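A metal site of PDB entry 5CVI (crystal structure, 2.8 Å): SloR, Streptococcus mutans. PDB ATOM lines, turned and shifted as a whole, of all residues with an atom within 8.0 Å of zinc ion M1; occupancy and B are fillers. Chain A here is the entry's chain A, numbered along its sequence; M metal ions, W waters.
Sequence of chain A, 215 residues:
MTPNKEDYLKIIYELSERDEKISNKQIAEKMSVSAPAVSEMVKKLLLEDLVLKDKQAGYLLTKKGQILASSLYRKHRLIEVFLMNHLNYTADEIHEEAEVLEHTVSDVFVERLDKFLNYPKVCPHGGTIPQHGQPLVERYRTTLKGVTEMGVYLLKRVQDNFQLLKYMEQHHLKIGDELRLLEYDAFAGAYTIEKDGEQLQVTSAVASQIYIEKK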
ATOM      1  N   LYS A  10      36.413  21.822  20.686  1.00  0.00           N
ATOM      2  CA  LYS A  10      36.027  22.357  19.387  1.00  0.00           C
ATOM      3  C   LYS A  10      36.779  23.639  19.071  1.00  0.00           C
ATOM      4  O   LYS A  10      37.050  23.938  17.907  1.00  0.00           O
ATOM      5  CB  LYS A  10      34.512  22.595  19.326  1.00  0.00           C
ATOM      6  CG  LYS A  10      33.681  21.325  19.455  1.00  0.00           C
ATOM      7  CD  LYS A  10      32.227  21.561  19.096  1.00  0.00           C
ATOM      8  CE  LYS A  10      31.588  22.614  20.004  1.00  0.00           C
ATOM      9  NZ  LYS A  10      30.220  22.983  19.539  1.00  0.00           N
ATOM     10  N   TYR A  73      30.818  17.561  16.548  1.00  0.00           N
ATOM     11  CA  TYR A  73      30.485  18.190  15.280  1.00  0.00           C
ATOM     12  C   TYR A  73      29.353  17.456  14.569  1.00  0.00           C
ATOM     13  O   TYR A  73      28.477  18.084  13.960  1.00  0.00           O
ATOM     14  CB  TYR A  73      31.718  18.305  14.378  1.00  0.00           C
ATOM     15  CG  TYR A  73      32.666  19.405  14.767  1.00  0.00           C
ATOM     16  CD1 TYR A  73      32.297  20.743  14.654  1.00  0.00           C
ATOM     17  CD2 TYR A  73      33.939  19.116  15.245  1.00  0.00           C
ATOM     18  CE1 TYR A  73      33.163  21.756  15.013  1.00  0.00           C
ATOM     19  CE2 TYR A  73      34.811  20.127  15.610  1.00  0.00           C
ATOM     20  CZ  TYR A  73      34.418  21.444  15.485  1.00  0.00           C
ATOM     21  OH  TYR A  73      35.276  22.454  15.848  1.00  0.00           O
ATOM     22  N   HIS A  76      26.106  18.388  16.448  1.00  0.00           N
ATOM     23  CA  HIS A  76      25.830  19.796  16.175  1.00  0.00           C
ATOM     24  C   HIS A  76      25.275  20.006  14.778  1.00  0.00           C
ATOM     25  O   HIS A  76      24.275  20.706  14.599  1.00  0.00           O
ATOM     26  CB  HIS A  76      27.112  20.612  16.355  1.00  0.00           C
ATOM     27  CG  HIS A  76      26.867  22.085  16.487  1.00  0.00           C
ATOM     28  ND1 HIS A  76      26.490  22.666  17.680  1.00  0.00           N
ATOM     29  CD2 HIS A  76      26.963  23.091  15.591  1.00  0.00           C
ATOM     30  CE1 HIS A  76      26.351  23.971  17.499  1.00  0.00           C
ATOM     31  NE2 HIS A  76      26.637  24.249  16.246  1.00  0.00           N
ATOM     32  N   ARG A  77      25.909  19.371  13.795  1.00  0.00           N
ATOM     33  CA  ARG A  77      25.547  19.595  12.405  1.00  0.00           C
ATOM     34  C   ARG A  77      24.244  18.909  11.977  1.00  0.00           C
ATOM     35  O   ARG A  77      23.452  19.485  11.225  1.00  0.00           O
ATOM     36  CB  ARG A  77      26.712  19.226  11.479  1.00  0.00           C
ATOM     37  CG  ARG A  77      27.880  20.198  11.582  1.00  0.00           C
ATOM     38  CD  ARG A  77      29.053  19.805  10.709  1.00  0.00           C
ATOM     39  NE  ARG A  77      30.093  20.844  10.726  1.00  0.00           N
ATOM     40  CZ  ARG A  77      31.359  20.636  10.398  1.00  0.00           C
ATOM     41  NH1 ARG A  77      31.773  19.428  10.031  1.00  0.00           N
ATOM     42  NH2 ARG A  77      32.232  21.634  10.446  1.00  0.00           N
ATOM     43  N   GLU A  80      21.659  21.042  13.152  1.00  0.00           N
ATOM     44  CA  GLU A  80      21.548  22.246  12.340  1.00  0.00           C
ATOM     45  C   GLU A  80      20.684  22.011  11.109  1.00  0.00           C
ATOM     46  O   GLU A  80      19.848  22.839  10.744  1.00  0.00           O
ATOM     47  CB  GLU A  80      22.924  22.771  11.928  1.00  0.00           C
ATOM     48  CG  GLU A  80      23.694  23.466  13.039  1.00  0.00           C
ATOM     49  CD  GLU A  80      25.045  23.984  12.564  1.00  0.00           C
ATOM     50  OE1 GLU A  80      25.638  24.831  13.268  1.00  0.00           O
ATOM     51  OE2 GLU A  80      25.500  23.552  11.481  1.00  0.00           O
ATOM     52  N   ALA A  91      19.781  31.548  10.262  1.00  0.00           N
ATOM     53  CA  ALA A  91      21.186  31.335  10.603  1.00  0.00           C
ATOM     54  C   ALA A  91      21.579  31.958  11.951  1.00  0.00           C
ATOM     55  O   ALA A  91      22.507  31.482  12.611  1.00  0.00           O
ATOM     56  CB  ALA A  91      22.084  31.860   9.495  1.00  0.00           C
ATOM     57  N   ILE A  94      20.263  29.308  15.054  1.00  0.00           N
ATOM     58  CA  ILE A  94      20.549  27.883  15.136  1.00  0.00           C
ATOM     59  C   ILE A  94      21.642  27.471  16.128  1.00  0.00           C
ATOM     60  O   ILE A  94      21.631  26.357  16.629  1.00  0.00           O
ATOM     61  CB  ILE A  94      20.886  27.278  13.750  1.00  0.00           C
ATOM     62  CG1 ILE A  94      22.063  28.033  13.128  1.00  0.00           C
ATOM     63  CG2 ILE A  94      19.672  27.303  12.842  1.00  0.00           C
ATOM     64  CD1 ILE A  94      22.545  27.447  11.817  1.00  0.00           C
ATOM     65  N   HIS A  95      22.587  28.368  16.405  1.00  0.00           N
ATOM     66  CA  HIS A  95      23.747  27.974  17.199  1.00  0.00           C
ATOM     67  C   HIS A  95      23.422  27.608  18.642  1.00  0.00           C
ATOM     68  O   HIS A  95      23.682  26.480  19.072  1.00  0.00           O
ATOM     69  CB  HIS A  95      24.857  29.022  17.173  1.00  0.00           C
ATOM     70  CG  HIS A  95      26.085  28.598  17.912  1.00  0.00           C
ATOM     71  ND1 HIS A  95      26.877  27.560  17.478  1.00  0.00           N
ATOM     72  CD2 HIS A  95      26.645  29.053  19.059  1.00  0.00           C
ATOM     73  CE1 HIS A  95      27.876  27.386  18.325  1.00  0.00           C
ATOM     74  NE2 HIS A  95      27.763  28.288  19.291  1.00  0.00           N
ATOM     75  N   GLU A  96      22.867  28.547  19.397  1.00  0.00           N
ATOM     76  CA  GLU A  96      22.600  28.325  20.817  1.00  0.00           C
ATOM     77  C   GLU A  96      21.659  27.139  21.015  1.00  0.00           C
ATOM     78  O   GLU A  96      21.783  26.390  21.982  1.00  0.00           O
ATOM     79  CB  GLU A  96      22.056  29.593  21.478  1.00  0.00           C
ATOM     80  CG  GLU A  96      22.033  29.549  23.001  1.00  0.00           C
ATOM     81  CD  GLU A  96      23.412  29.302  23.609  1.00  0.00           C
ATOM     82  OE1 GLU A  96      23.478  28.685  24.700  1.00  0.00           O
ATOM     83  OE2 GLU A  96      24.425  29.721  23.003  1.00  0.00           O
ATOM     84  N   GLU A  97      20.711  26.974  20.098  1.00  0.00           N
ATOM     85  CA  GLU A  97      19.789  25.840  20.150  1.00  0.00           C
ATOM     86  C   GLU A  97      20.545  24.532  19.933  1.00  0.00           C
ATOM     87  O   GLU A  97      20.407  23.579  20.707  1.00  0.00           O
ATOM     88  CB  GLU A  97      18.688  25.983  19.107  1.00  0.00           C
ATOM     89  CG  GLU A  97      17.508  25.053  19.328  1.00  0.00           C
ATOM     90  CD  GLU A  97      16.617  25.511  20.476  1.00  0.00           C
ATOM     91  OE1 GLU A  97      15.876  26.501  20.293  1.00  0.00           O
ATOM     92  OE2 GLU A  97      16.678  24.888  21.555  1.00  0.00           O
ATOM     93  N   ALA A  98      21.342  24.492  18.867  1.00  0.00           N
ATOM     94  CA  ALA A  98      22.123  23.306  18.524  1.00  0.00           C
ATOM     95  C   ALA A  98      23.204  23.047  19.569  1.00  0.00           C
ATOM     96  O   ALA A  98      23.619  21.923  19.788  1.00  0.00           O
ATOM     97  CB  ALA A  98      22.747  23.461  17.146  1.00  0.00           C
ATOM     98  N   GLU A  99      23.649  24.122  20.196  1.00  0.00           N
ATOM     99  CA  GLU A  99      24.676  24.056  21.220  1.00  0.00           C
ATOM    100  C   GLU A  99      24.165  23.344  22.464  1.00  0.00           C
ATOM    101  O   GLU A  99      24.870  22.499  23.028  1.00  0.00           O
ATOM    102  CB  GLU A  99      25.152  25.480  21.582  1.00  0.00           C
ATOM    103  CG  GLU A  99      26.213  25.534  22.648  1.00  0.00           C
ATOM    104  CD  GLU A  99      27.377  24.610  22.349  1.00  0.00           C
ATOM    105  OE1 GLU A  99      27.722  24.464  21.151  1.00  0.00           O
ATOM    106  OE2 GLU A  99      27.930  24.024  23.299  1.00  0.00           O
ATOM    107  N   GLU A 102      23.301  19.388  21.617  1.00  0.00           N
ATOM    108  CA  GLU A 102      24.437  18.490  21.393  1.00  0.00           C
ATOM    109  C   GLU A 102      24.962  17.935  22.730  1.00  0.00           C
ATOM    110  O   GLU A 102      25.645  16.917  22.748  1.00  0.00           O
ATOM    111  CB  GLU A 102      25.561  19.193  20.633  1.00  0.00           C
ATOM    112  CG  GLU A 102      26.403  20.137  21.489  1.00  0.00           C
ATOM    113  CD  GLU A 102      27.584  20.732  20.738  1.00  0.00           C
ATOM    114  OE1 GLU A 102      27.640  20.595  19.501  1.00  0.00           O
ATOM    115  OE2 GLU A 102      28.454  21.325  21.402  1.00  0.00           O
ATOM    116  N   HIS A 125      26.757  25.218   6.997  1.00  0.00           N
ATOM    117  CA  HIS A 125      28.004  25.956   6.799  1.00  0.00           C
ATOM    118  C   HIS A 125      28.875  25.323   5.726  1.00  0.00           C
ATOM    119  O   HIS A 125      29.925  25.858   5.376  1.00  0.00           O
ATOM    120  CB  HIS A 125      28.793  26.059   8.113  1.00  0.00           C
ATOM    121  CG  HIS A 125      28.022  26.693   9.237  1.00  0.00           C
ATOM    122  ND1 HIS A 125      27.294  25.959  10.139  1.00  0.00           N
ATOM    123  CD2 HIS A 125      27.875  27.988   9.601  1.00  0.00           C
ATOM    124  CE1 HIS A 125      26.736  26.771  11.014  1.00  0.00           C
ATOM    125  NE2 HIS A 125      27.073  28.009  10.704  1.00  0.00           N
ATOM    126  N   GLN A 159      33.226  28.949   8.551  1.00  0.00           N
ATOM    127  CA  GLN A 159      33.284  28.610   9.966  1.00  0.00           C
ATOM    128  C   GLN A 159      31.955  28.934  10.634  1.00  0.00           C
ATOM    129  O   GLN A 159      31.250  29.852  10.218  1.00  0.00           O
ATOM    130  CB  GLN A 159      34.391  29.396  10.677  1.00  0.00           C
ATOM    131  CG  GLN A 159      35.803  28.933  10.364  1.00  0.00           C
ATOM    132  CD  GLN A 159      36.175  27.646  11.062  1.00  0.00           C
ATOM    133  OE1 GLN A 159      35.315  26.867  11.463  1.00  0.00           O
ATOM    134  NE2 GLN A 159      37.481  27.417  11.223  1.00  0.00           N
ATOM    135  N   ASP A 160      31.622  28.158  11.650  1.00  0.00           N
ATOM    136  CA  ASP A 160      30.517  28.477  12.534  1.00  0.00           C
ATOM    137  C   ASP A 160      30.968  29.652  13.396  1.00  0.00           C
ATOM    138  O   ASP A 160      31.654  29.463  14.404  1.00  0.00           O
ATOM    139  CB  ASP A 160      30.193  27.275  13.414  1.00  0.00           C
ATOM    140  CG  ASP A 160      28.887  27.418  14.160  1.00  0.00           C
ATOM    141  OD1 ASP A 160      28.416  28.555  14.332  1.00  0.00           O
ATOM    142  OD2 ASP A 160      28.339  26.379  14.569  1.00  0.00           O
ATOM    143  N   ASN A 161      30.611  30.863  12.997  1.00  0.00           N
ATOM    144  CA  ASN A 161      31.001  32.053  13.739  1.00  0.00           C
ATOM    145  C   ASN A 161      29.941  33.142  13.576  1.00  0.00           C
ATOM    146  O   ASN A 161      29.481  33.392  12.466  1.00  0.00           O
ATOM    147  CB  ASN A 161      32.360  32.566  13.255  1.00  0.00           C
ATOM    148  CG  ASN A 161      32.897  33.711  14.088  1.00  0.00           C
ATOM    149  OD1 ASN A 161      32.425  34.841  14.001  1.00  0.00           O
ATOM    150  ND2 ASN A 161      33.892  33.419  14.922  1.00  0.00           N
HETATM  151 ZN    ZN M   1      26.925  26.243  15.941  1.00  0.00          ZN
HETATM  152 ZN    ZN M   2      27.311  23.912  10.670  1.00  0.00          ZN
HETATM  153  O   HOH W   1      25.373  26.827  14.638  1.00  0.00           O
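OE1 of Glu 80 lies close to NE2 of His 76 (3.2 Å).
A ring nitrogen (ND1) of His 76 is in hydrogen-bond range of the side-chain carboxylate (OE1) of Glu 102.
Merely in contact with zinc ion M1: Glu 80.
Within 4 Å of zinc ion M1: His 76, Glu 80, His 95 and Asp 160.
The nearest printed residue that does not touch zinc ion M1 is His 125 (5.0 Å).
Zinc ion M1 is bound by the side-chain carboxylate of Asp 160, a ring nitrogen (ND1) of His 95, a ring nitrogen (NE2) of His 76 and water W1.
Zinc ion M1 has four donor atoms within binding distance.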
